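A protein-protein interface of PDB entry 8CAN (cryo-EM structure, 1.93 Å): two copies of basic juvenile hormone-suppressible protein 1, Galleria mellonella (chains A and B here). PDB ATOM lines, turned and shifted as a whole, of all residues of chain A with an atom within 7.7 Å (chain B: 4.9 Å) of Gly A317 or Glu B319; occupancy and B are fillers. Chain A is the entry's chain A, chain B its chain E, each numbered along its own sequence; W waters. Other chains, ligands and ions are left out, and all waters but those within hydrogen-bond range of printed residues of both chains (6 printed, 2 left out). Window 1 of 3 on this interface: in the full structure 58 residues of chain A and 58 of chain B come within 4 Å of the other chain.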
ATOM      1  N   GLY A 101      15.045 -10.373 -12.845  1.00  0.00           N
ATOM      2  CA  GLY A 101      14.493  -9.696 -11.691  1.00  0.00           C
ATOM      3  C   GLY A 101      15.092  -8.346 -11.379  1.00  0.00           C
ATOM      4  O   GLY A 101      14.744  -7.752 -10.356  1.00  0.00           O
ATOM      5  N   VAL A 103      16.530  -4.350 -13.113  1.00  0.00           N
ATOM      6  CA  VAL A 103      16.106  -3.312 -14.045  1.00  0.00           C
ATOM      7  C   VAL A 103      17.244  -3.024 -15.013  1.00  0.00           C
ATOM      8  O   VAL A 103      18.401  -2.877 -14.601  1.00  0.00           O
ATOM      9  CB  VAL A 103      15.680  -2.029 -13.306  1.00  0.00           C
ATOM     10  CG1 VAL A 103      15.242  -0.963 -14.300  1.00  0.00           C
ATOM     11  CG2 VAL A 103      14.566  -2.331 -12.316  1.00  0.00           C
ATOM     12  N   TYR A 173       5.913  -1.545 -21.573  1.00  0.00           N
ATOM     13  CA  TYR A 173       6.426  -1.371 -20.215  1.00  0.00           C
ATOM     14  C   TYR A 173       5.860  -0.074 -19.651  1.00  0.00           C
ATOM     15  O   TYR A 173       6.538   0.963 -19.640  1.00  0.00           O
ATOM     16  CB  TYR A 173       7.956  -1.373 -20.208  1.00  0.00           C
ATOM     17  CG  TYR A 173       8.577  -1.631 -18.853  1.00  0.00           C
ATOM     18  CD1 TYR A 173       8.429  -2.860 -18.222  1.00  0.00           C
ATOM     19  CD2 TYR A 173       9.331  -0.656 -18.214  1.00  0.00           C
ATOM     20  CE1 TYR A 173       8.999  -3.103 -16.988  1.00  0.00           C
ATOM     21  CE2 TYR A 173       9.907  -0.892 -16.980  1.00  0.00           C
ATOM     22  CZ  TYR A 173       9.738  -2.117 -16.372  1.00  0.00           C
ATOM     23  OH  TYR A 173      10.309  -2.356 -15.143  1.00  0.00           O
ATOM     24  N   TYR A 175       5.553   0.953 -16.773  1.00  0.00           N
ATOM     25  CA  TYR A 175       6.191   1.429 -15.550  1.00  0.00           C
ATOM     26  C   TYR A 175       6.964   2.723 -15.778  1.00  0.00           C
ATOM     27  O   TYR A 175       6.991   3.601 -14.907  1.00  0.00           O
ATOM     28  CB  TYR A 175       7.121   0.346 -14.999  1.00  0.00           C
ATOM     29  CG  TYR A 175       6.397  -0.815 -14.358  1.00  0.00           C
ATOM     30  CD1 TYR A 175       6.104  -0.810 -13.002  1.00  0.00           C
ATOM     31  CD2 TYR A 175       6.007  -1.916 -15.108  1.00  0.00           C
ATOM     32  CE1 TYR A 175       5.443  -1.868 -12.409  1.00  0.00           C
ATOM     33  CE2 TYR A 175       5.345  -2.978 -14.525  1.00  0.00           C
ATOM     34  CZ  TYR A 175       5.066  -2.949 -13.175  1.00  0.00           C
ATOM     35  OH  TYR A 175       4.407  -4.005 -12.589  1.00  0.00           O
ATOM     36  N   SER A 180       3.202   6.188 -10.456  1.00  0.00           N
ATOM     37  CA  SER A 180       3.200   5.018  -9.584  1.00  0.00           C
ATOM     38  C   SER A 180       1.832   4.785  -8.953  1.00  0.00           C
ATOM     39  O   SER A 180       1.401   3.636  -8.801  1.00  0.00           O
ATOM     40  CB  SER A 180       4.266   5.178  -8.502  1.00  0.00           C
ATOM     41  OG  SER A 180       4.065   6.369  -7.761  1.00  0.00           O
ATOM     42  N   HIS A 224       3.181  16.705  -5.661  1.00  0.00           N
ATOM     43  CA  HIS A 224       4.591  16.428  -5.909  1.00  0.00           C
ATOM     44  C   HIS A 224       5.353  17.668  -6.358  1.00  0.00           C
ATOM     45  O   HIS A 224       6.469  17.545  -6.874  1.00  0.00           O
ATOM     46  CB  HIS A 224       4.737  15.324  -6.960  1.00  0.00           C
ATOM     47  CG  HIS A 224       3.975  14.077  -6.639  1.00  0.00           C
ATOM     48  ND1 HIS A 224       2.708  13.834  -7.125  1.00  0.00           N
ATOM     49  CD2 HIS A 224       4.300  13.001  -5.884  1.00  0.00           C
ATOM     50  CE1 HIS A 224       2.286  12.662  -6.684  1.00  0.00           C
ATOM     51  NE2 HIS A 224       3.234  12.137  -5.928  1.00  0.00           N
ATOM     52  N   TRP A 309      10.467  15.366  -8.740  1.00  0.00           N
ATOM     53  CA  TRP A 309       9.869  14.167  -8.160  1.00  0.00           C
ATOM     54  C   TRP A 309       9.507  13.203  -9.287  1.00  0.00           C
ATOM     55  O   TRP A 309       8.527  13.439 -10.010  1.00  0.00           O
ATOM     56  CB  TRP A 309       8.625  14.530  -7.344  1.00  0.00           C
ATOM     57  CG  TRP A 309       8.193  13.472  -6.372  1.00  0.00           C
ATOM     58  CD1 TRP A 309       7.942  12.159  -6.646  1.00  0.00           C
ATOM     59  CD2 TRP A 309       7.946  13.644  -4.971  1.00  0.00           C
ATOM     60  NE1 TRP A 309       7.562  11.501  -5.501  1.00  0.00           N
ATOM     61  CE2 TRP A 309       7.556  12.391  -4.459  1.00  0.00           C
ATOM     62  CE3 TRP A 309       8.019  14.735  -4.100  1.00  0.00           C
ATOM     63  CZ2 TRP A 309       7.242  12.199  -3.116  1.00  0.00           C
ATOM     64  CZ3 TRP A 309       7.707  14.542  -2.767  1.00  0.00           C
ATOM     65  CH2 TRP A 309       7.323  13.283  -2.289  1.00  0.00           C
ATOM     66  N   ILE A 312       7.953   7.527 -10.553  1.00  0.00           N
ATOM     67  CA  ILE A 312       8.149   6.380 -11.435  1.00  0.00           C
ATOM     68  C   ILE A 312       8.380   5.146 -10.574  1.00  0.00           C
ATOM     69  O   ILE A 312       9.248   5.149  -9.692  1.00  0.00           O
ATOM     70  CB  ILE A 312       9.323   6.596 -12.403  1.00  0.00           C
ATOM     71  CG1 ILE A 312       8.995   7.701 -13.413  1.00  0.00           C
ATOM     72  CG2 ILE A 312       9.672   5.297 -13.118  1.00  0.00           C
ATOM     73  CD1 ILE A 312       7.843   7.378 -14.352  1.00  0.00           C
ATOM     74  N   LEU A 313       7.607   4.096 -10.834  1.00  0.00           N
ATOM     75  CA  LEU A 313       7.755   2.813 -10.165  1.00  0.00           C
ATOM     76  C   LEU A 313       8.428   1.819 -11.102  1.00  0.00           C
ATOM     77  O   LEU A 313       8.116   1.767 -12.295  1.00  0.00           O
ATOM     78  CB  LEU A 313       6.394   2.270  -9.721  1.00  0.00           C
ATOM     79  CG  LEU A 313       6.375   0.863  -9.115  1.00  0.00           C
ATOM     80  CD1 LEU A 313       7.164   0.819  -7.817  1.00  0.00           C
ATOM     81  CD2 LEU A 313       4.944   0.399  -8.892  1.00  0.00           C
ATOM     82  N   LEU A 314       9.353   1.039 -10.557  1.00  0.00           N
ATOM     83  CA  LEU A 314      10.029  -0.017 -11.295  1.00  0.00           C
ATOM     84  C   LEU A 314       9.453  -1.370 -10.898  1.00  0.00           C
ATOM     85  O   LEU A 314       8.949  -1.548  -9.787  1.00  0.00           O
ATOM     86  CB  LEU A 314      11.536   0.016 -11.032  1.00  0.00           C
ATOM     87  CG  LEU A 314      12.228   1.344 -11.351  1.00  0.00           C
ATOM     88  CD1 LEU A 314      13.673   1.335 -10.876  1.00  0.00           C
ATOM     89  CD2 LEU A 314      12.154   1.644 -12.840  1.00  0.00           C
ATOM     90  N   HIS A 315       9.534  -2.331 -11.822  1.00  0.00           N
ATOM     91  CA  HIS A 315       8.944  -3.642 -11.579  1.00  0.00           C
ATOM     92  C   HIS A 315       9.628  -4.392 -10.443  1.00  0.00           C
ATOM     93  O   HIS A 315       9.078  -5.391  -9.965  1.00  0.00           O
ATOM     94  CB  HIS A 315       8.985  -4.487 -12.856  1.00  0.00           C
ATOM     95  CG  HIS A 315      10.352  -4.972 -13.222  1.00  0.00           C
ATOM     96  ND1 HIS A 315      11.233  -4.224 -13.973  1.00  0.00           N
ATOM     97  CD2 HIS A 315      10.985  -6.138 -12.950  1.00  0.00           C
ATOM     98  CE1 HIS A 315      12.353  -4.904 -14.141  1.00  0.00           C
ATOM     99  NE2 HIS A 315      12.228  -6.069 -13.530  1.00  0.00           N
ATOM    100  N   THR A 316      10.802  -3.941 -10.001  1.00  0.00           N
ATOM    101  CA  THR A 316      11.464  -4.528  -8.844  1.00  0.00           C
ATOM    102  C   THR A 316      10.848  -4.084  -7.522  1.00  0.00           C
ATOM    103  O   THR A 316      11.181  -4.662  -6.482  1.00  0.00           O
ATOM    104  CB  THR A 316      12.951  -4.167  -8.850  1.00  0.00           C
ATOM    105  OG1 THR A 316      13.100  -2.742  -8.874  1.00  0.00           O
ATOM    106  CG2 THR A 316      13.641  -4.770 -10.062  1.00  0.00           C
ATOM    107  N   GLY A 317       9.970  -3.084  -7.536  1.00  0.00           N
ATOM    108  CA  GLY A 317       9.348  -2.579  -6.331  1.00  0.00           C
ATOM    109  C   GLY A 317       9.944  -1.298  -5.788  1.00  0.00           C
ATOM    110  O   GLY A 317       9.470  -0.807  -4.755  1.00  0.00           O
ATOM    111  N   ASP A 318      10.959  -0.743  -6.443  1.00  0.00           N
ATOM    112  CA  ASP A 318      11.598   0.492  -6.017  1.00  0.00           C
ATOM    113  C   ASP A 318      11.259   1.618  -6.985  1.00  0.00           C
ATOM    114  O   ASP A 318      11.097   1.398  -8.188  1.00  0.00           O
ATOM    115  CB  ASP A 318      13.119   0.324  -5.933  1.00  0.00           C
ATOM    116  CG  ASP A 318      13.537  -0.684  -4.880  1.00  0.00           C
ATOM    117  OD1 ASP A 318      12.860  -0.770  -3.835  1.00  0.00           O
ATOM    118  OD2 ASP A 318      14.544  -1.389  -5.098  1.00  0.00           O
ATOM    119  N   GLU A 319      11.151   2.829  -6.446  1.00  0.00           N
ATOM    120  CA  GLU A 319      10.863   4.018  -7.232  1.00  0.00           C
ATOM    121  C   GLU A 319      12.135   4.823  -7.464  1.00  0.00           C
ATOM    122  O   GLU A 319      13.095   4.741  -6.692  1.00  0.00           O
ATOM    123  CB  GLU A 319       9.823   4.899  -6.535  1.00  0.00           C
ATOM    124  CG  GLU A 319       8.417   4.325  -6.523  1.00  0.00           C
ATOM    125  CD  GLU A 319       7.391   5.321  -6.019  1.00  0.00           C
ATOM    126  OE1 GLU A 319       7.782   6.456  -5.673  1.00  0.00           O
ATOM    127  OE2 GLU A 319       6.193   4.972  -5.970  1.00  0.00           O
ATOM    128  N   MET A 320      12.132   5.603  -8.537  1.00  0.00           N
ATOM    129  CA  MET A 320      13.255   6.484  -8.815  1.00  0.00           C
ATOM    130  C   MET A 320      13.381   7.516  -7.696  1.00  0.00           C
ATOM    131  O   MET A 320      12.370   8.105  -7.288  1.00  0.00           O
ATOM    132  CB  MET A 320      13.073   7.184 -10.161  1.00  0.00           C
ATOM    133  CG  MET A 320      13.212   6.263 -11.362  1.00  0.00           C
ATOM    134  SD  MET A 320      13.141   7.153 -12.930  1.00  0.00           S
ATOM    135  CE  MET A 320      13.578   5.852 -14.081  1.00  0.00           C
ATOM    136  N   PRO A 321      14.582   7.762  -7.176  1.00  0.00           N
ATOM    137  CA  PRO A 321      14.711   8.663  -6.026  1.00  0.00           C
ATOM    138  C   PRO A 321      14.358  10.100  -6.376  1.00  0.00           C
ATOM    139  O   PRO A 321      14.511  10.549  -7.515  1.00  0.00           O
ATOM    140  CB  PRO A 321      16.188   8.532  -5.638  1.00  0.00           C
ATOM    141  CG  PRO A 321      16.870   8.126  -6.891  1.00  0.00           C
ATOM    142  CD  PRO A 321      15.891   7.272  -7.642  1.00  0.00           C
ATOM    143  N   VAL A 322      13.880  10.822  -5.367  1.00  0.00           N
ATOM    144  CA  VAL A 322      13.554  12.237  -5.488  1.00  0.00           C
ATOM    145  C   VAL A 322      14.802  13.056  -5.193  1.00  0.00           C
ATOM    146  O   VAL A 322      15.587  12.718  -4.301  1.00  0.00           O
ATOM    147  CB  VAL A 322      12.404  12.615  -4.533  1.00  0.00           C
ATOM    148  CG1 VAL A 322      12.151  14.115  -4.563  1.00  0.00           C
ATOM    149  CG2 VAL A 322      11.139  11.848  -4.891  1.00  0.00           C
ATOM    150  N   TYR A 491       0.194  -8.680 -13.219  1.00  0.00           N
ATOM    151  CA  TYR A 491       0.641 -10.060 -13.353  1.00  0.00           C
ATOM    152  C   TYR A 491      -0.561 -10.986 -13.484  1.00  0.00           C
ATOM    153  O   TYR A 491      -1.575 -10.807 -12.802  1.00  0.00           O
ATOM    154  CB  TYR A 491       1.500 -10.468 -12.156  1.00  0.00           C
ATOM    155  CG  TYR A 491       2.870  -9.829 -12.155  1.00  0.00           C
ATOM    156  CD1 TYR A 491       3.023  -8.465 -11.933  1.00  0.00           C
ATOM    157  CD2 TYR A 491       4.012 -10.587 -12.373  1.00  0.00           C
ATOM    158  CE1 TYR A 491       4.272  -7.877 -11.934  1.00  0.00           C
ATOM    159  CE2 TYR A 491       5.266 -10.007 -12.374  1.00  0.00           C
ATOM    160  CZ  TYR A 491       5.390  -8.652 -12.154  1.00  0.00           C
ATOM    161  OH  TYR A 491       6.638  -8.070 -12.153  1.00  0.00           O
ATOM    162  N   SER B 180       9.419  -1.552   0.651  1.00  0.00           N
ATOM    163  CA  SER B 180       8.458  -1.476  -0.446  1.00  0.00           C
ATOM    164  C   SER B 180       8.560  -2.684  -1.371  1.00  0.00           C
ATOM    165  O   SER B 180       7.541  -3.184  -1.860  1.00  0.00           O
ATOM    166  CB  SER B 180       8.669  -0.183  -1.232  1.00  0.00           C
ATOM    167  OG  SER B 180      10.000  -0.089  -1.709  1.00  0.00           O
ATOM    168  N   ASN B 181       9.779  -3.157  -1.640  1.00  0.00           N
ATOM    169  CA  ASN B 181       9.950  -4.248  -2.596  1.00  0.00           C
ATOM    170  C   ASN B 181       9.283  -5.527  -2.102  1.00  0.00           C
ATOM    171  O   ASN B 181       8.713  -6.288  -2.896  1.00  0.00           O
ATOM    172  CB  ASN B 181      11.437  -4.484  -2.864  1.00  0.00           C
ATOM    173  CG  ASN B 181      12.186  -4.952  -1.633  1.00  0.00           C
ATOM    174  OD1 ASN B 181      12.263  -6.148  -1.356  1.00  0.00           O
ATOM    175  ND2 ASN B 181      12.749  -4.009  -0.889  1.00  0.00           N
ATOM    176  N   HIS B 184       5.683  -5.207  -2.756  1.00  0.00           N
ATOM    177  CA  HIS B 184       5.443  -5.348  -4.189  1.00  0.00           C
ATOM    178  C   HIS B 184       5.442  -6.815  -4.601  1.00  0.00           C
ATOM    179  O   HIS B 184       4.600  -7.248  -5.396  1.00  0.00           O
ATOM    180  CB  HIS B 184       6.502  -4.570  -4.971  1.00  0.00           C
ATOM    181  CG  HIS B 184       6.299  -4.592  -6.453  1.00  0.00           C
ATOM    182  ND1 HIS B 184       5.266  -3.924  -7.074  1.00  0.00           N
ATOM    183  CD2 HIS B 184       7.001  -5.198  -7.439  1.00  0.00           C
ATOM    184  CE1 HIS B 184       5.339  -4.120  -8.379  1.00  0.00           C
ATOM    185  NE2 HIS B 184       6.383  -4.890  -8.626  1.00  0.00           N
ATOM    186  N   ILE B 312       9.993   3.167   1.984  1.00  0.00           N
ATOM    187  CA  ILE B 312       8.678   3.041   2.606  1.00  0.00           C
ATOM    188  C   ILE B 312       7.619   3.332   1.553  1.00  0.00           C
ATOM    189  O   ILE B 312       7.667   4.372   0.884  1.00  0.00           O
ATOM    190  CB  ILE B 312       8.521   3.982   3.811  1.00  0.00           C
ATOM    191  CG1 ILE B 312       9.441   3.551   4.959  1.00  0.00           C
ATOM    192  CG2 ILE B 312       7.069   4.027   4.270  1.00  0.00           C
ATOM    193  CD1 ILE B 312       9.112   2.191   5.553  1.00  0.00           C
ATOM    194  N   LEU B 313       6.665   2.417   1.412  1.00  0.00           N
ATOM    195  CA  LEU B 313       5.532   2.580   0.513  1.00  0.00           C
ATOM    196  C   LEU B 313       4.284   2.919   1.317  1.00  0.00           C
ATOM    197  O   LEU B 313       4.043   2.344   2.382  1.00  0.00           O
ATOM    198  CB  LEU B 313       5.295   1.306  -0.302  1.00  0.00           C
ATOM    199  CG  LEU B 313       4.055   1.281  -1.200  1.00  0.00           C
ATOM    200  CD1 LEU B 313       4.151   2.334  -2.292  1.00  0.00           C
ATOM    201  CD2 LEU B 313       3.861  -0.103  -1.801  1.00  0.00           C
ATOM    202  N   LEU B 314       3.498   3.859   0.805  1.00  0.00           N
ATOM    203  CA  LEU B 314       2.229   4.240   1.405  1.00  0.00           C
ATOM    204  C   LEU B 314       1.081   3.633   0.607  1.00  0.00           C
ATOM    205  O   LEU B 314       1.204   3.376  -0.593  1.00  0.00           O
ATOM    206  CB  LEU B 314       2.088   5.763   1.459  1.00  0.00           C
ATOM    207  CG  LEU B 314       3.210   6.497   2.199  1.00  0.00           C
ATOM    208  CD1 LEU B 314       3.081   8.002   2.032  1.00  0.00           C
ATOM    209  CD2 LEU B 314       3.217   6.121   3.674  1.00  0.00           C
ATOM    210  N   GLY B 317       0.010   4.715  -2.884  1.00  0.00           N
ATOM    211  CA  GLY B 317       0.830   4.437  -4.043  1.00  0.00           C
ATOM    212  C   GLY B 317       2.090   5.267  -4.154  1.00  0.00           C
ATOM    213  O   GLY B 317       2.841   5.090  -5.123  1.00  0.00           O
ATOM    214  N   ASP B 318       2.348   6.160  -3.204  1.00  0.00           N
ATOM    215  CA  ASP B 318       3.534   7.002  -3.205  1.00  0.00           C
ATOM    216  C   ASP B 318       4.484   6.570  -2.095  1.00  0.00           C
ATOM    217  O   ASP B 318       4.057   6.119  -1.029  1.00  0.00           O
ATOM    218  CB  ASP B 318       3.162   8.477  -3.022  1.00  0.00           C
ATOM    219  CG  ASP B 318       2.332   9.016  -4.170  1.00  0.00           C
ATOM    220  OD1 ASP B 318       2.555   8.586  -5.321  1.00  0.00           O
ATOM    221  OD2 ASP B 318       1.457   9.871  -3.921  1.00  0.00           O
ATOM    222  N   GLU B 319       5.779   6.711  -2.358  1.00  0.00           N
ATOM    223  CA  GLU B 319       6.819   6.376  -1.398  1.00  0.00           C
ATOM    224  C   GLU B 319       7.364   7.639  -0.743  1.00  0.00           C
ATOM    225  O   GLU B 319       7.295   8.734  -1.307  1.00  0.00           O
ATOM    226  CB  GLU B 319       7.965   5.615  -2.069  1.00  0.00           C
ATOM    227  CG  GLU B 319       7.620   4.198  -2.489  1.00  0.00           C
ATOM    228  CD  GLU B 319       8.838   3.418  -2.949  1.00  0.00           C
ATOM    229  OE1 GLU B 319       9.947   3.992  -2.946  1.00  0.00           O
ATOM    230  OE2 GLU B 319       8.685   2.232  -3.311  1.00  0.00           O
ATOM    231  N   MET B 320       7.908   7.474   0.456  1.00  0.00           N
ATOM    232  CA  MET B 320       8.540   8.591   1.142  1.00  0.00           C
ATOM    233  C   MET B 320       9.742   9.069   0.331  1.00  0.00           C
ATOM    234  O   MET B 320      10.544   8.241  -0.124  1.00  0.00           O
ATOM    235  CB  MET B 320       8.978   8.181   2.548  1.00  0.00           C
ATOM    236  CG  MET B 320       7.827   7.951   3.514  1.00  0.00           C
ATOM    237  SD  MET B 320       8.390   7.620   5.194  1.00  0.00           S
ATOM    238  CE  MET B 320       6.836   7.651   6.087  1.00  0.00           C
ATOM    239  N   PRO B 321       9.906  10.375   0.128  1.00  0.00           N
ATOM    240  CA  PRO B 321      10.987  10.851  -0.739  1.00  0.00           C
ATOM    241  C   PRO B 321      12.364  10.578  -0.152  1.00  0.00           C
ATOM    242  O   PRO B 321      12.549  10.514   1.066  1.00  0.00           O
ATOM    243  CB  PRO B 321      10.719  12.356  -0.846  1.00  0.00           C
ATOM    244  CG  PRO B 321       9.976  12.694   0.393  1.00  0.00           C
ATOM    245  CD  PRO B 321       9.145  11.488   0.722  1.00  0.00           C
ATOM    246  N   ILE B 418       2.514  14.431   1.494  1.00  0.00           N
ATOM    247  CA  ILE B 418       3.265  13.179   1.497  1.00  0.00           C
ATOM    248  C   ILE B 418       4.291  13.257   2.629  1.00  0.00           C
ATOM    249  O   ILE B 418       5.186  14.112   2.574  1.00  0.00           O
ATOM    250  CB  ILE B 418       3.953  12.932   0.149  1.00  0.00           C
ATOM    251  CG1 ILE B 418       2.916  12.910  -0.978  1.00  0.00           C
ATOM    252  CG2 ILE B 418       4.732  11.621   0.180  1.00  0.00           C
ATOM    253  CD1 ILE B 418       3.512  12.799  -2.367  1.00  0.00           C
HETATM  254  O   HOH W   1       6.804  -1.185  -4.027  1.00  0.00           O
HETATM  255  O   HOH W   2      12.744   2.594  -3.452  1.00  0.00           O
HETATM  256  O   HOH W   3       3.007   2.522  -6.442  1.00  0.00           O
HETATM  257  O   HOH W   4       2.775   8.992  -7.884  1.00  0.00           O
HETATM  258  O   HOH W   5       5.901   8.844  -5.002  1.00  0.00           O
HETATM  259  O   HOH W   6      12.642  -1.191  -1.280  1.00  0.00           O
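Of the 19 printed residues of chain A, 8 touch a printed residue of chain B. Hydrophobic or aromatic side chains of chain A that line the printed part of chain B: His A224 and Trp A309. Along chain A the printed residues that touch a printed residue of chain B span positions 180 to 319. Hydrophobic or aromatic side chains of chain B within 4 Å of the printed part of chain A: His B184, Pro B321 and Ile B418. Among the printed residues, 16 pairs touch across the chains. Among the printed residues, no Asp or Glu carboxylate lies within 4 Å of a Lys or Arg side-chain nitrogen of the other chain.
Ser A180 touches Gly B317, and with the chains exchanged Gly A317 touches Ser B180. Ser A180 touches Asp B318, and with the chains exchanged Asp A318 touches Ser B180. Gly A317 touches Glu B319, and with the chains exchanged Glu A319 touches Gly B317. Glu A319 touches its own counterpart, Glu B319. Of the 16 pairs that touch across the chains among the printed residues, 7 have their exchanged pair printed and touching as well.
Water W6 lies within hydrogen-bond range of OD1 of Asp A318, ND2 of Asn B181 and OG of Ser B180. Water W4 lies within hydrogen-bond range of the side-chain carboxylate of Asp B318 (2.6 Å) and the side-chain hydroxyl of Ser A180 (2.9 Å). Water W1 lies within hydrogen-bond range of O of Gly A317 and O of Ser B180. Water W3 lies within hydrogen-bond range of O of Gly B317 and O of Ser A180. Water W5 lies within hydrogen-bond range of OE1 of Glu A319 (3.1 Å), NE1 of Trp A309 (3.2 Å), OD1 of Asp B318 (3.4 Å) and N of Glu B319 (3.4 Å). Water W2 lies within hydrogen-bond range of the side-chain carboxylate (OE1) of Glu B319, the side-chain carboxylate (OD1) of Asp A318 and the backbone NH (N) of Glu A319.
The backbone NH (N) of His A315 lies close to the side-chain hydroxyl (OH) of Tyr A173 (3.4 Å). OG of Ser A180 sits at hydrogen-bond distance from OE2 of Glu A319, at 3.1 Å. OE2 of Glu B319 sits at hydrogen-bond distance from OG of Ser B180, 3.1 Å away.
OG of Ser A180 touches OD1 of Asp B318, 3.6 Å away. His A224 touches Asp B318 (NE2 to OD2, 3.5 Å). His A224 touches Ile B418. Trp A309 touches Glu B319. CB of Pro B321 touches CH2 of Trp A309, 3.8 Å away. CH2 of Trp A309 touches CD1 of Ile B418, at 3.8 Å. Asn B181 touches Thr A316 (CB to O, 3.6 Å). N of Asn B181 touches O of Gly A317, 3.9 Å away. Gly A317 touches His B184. Glu A319 touches Glu B319.
Val A103 touches none of the printed residues of chain B. Of the printed residues of chain B, Thr A316 touches Asn B181. Gly A317 touches just these residues of chain B: Ser B180, Asn B181, His B184 and Glu B319. Of the printed residues of chain B, Asp A318 touches Ser B180 (3.6 Å). Printed residues of chain A within 4 Å of Ser B180: Gly A317 and Asp A318. Leu B313 touches none of the printed residues of chain A. Of the printed residues of chain A, Asp B318 touches Ser A180 and His A224. Glu B319 touches just these residues of chain A: Trp A309 (3.9 Å), Gly A317 (3.5 Å) and Glu A319 (3.7 Å). The nearest printed residue of chain B that does not touch Ser A180 is Glu B319 (5.7 Å).
The side-chain hydroxyl (OG) of Ser A180 is in hydrogen-bond range of the backbone carbonyl oxygen (O) of Gly B317 (3.2 Å). O of His A315 lies within hydrogen-bond range of NE2 of His B184, at 3.1 Å. The backbone carbonyl oxygen (O) of Gly A317 lies within hydrogen-bond range of the side-chain hydroxyl (OG) of Ser B180 (3.2 Å). OE2 of Glu B319 sits close to O of Gly A317. OE2 of Glu A319 sits close to O of Gly B317, at 3.5 Å.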
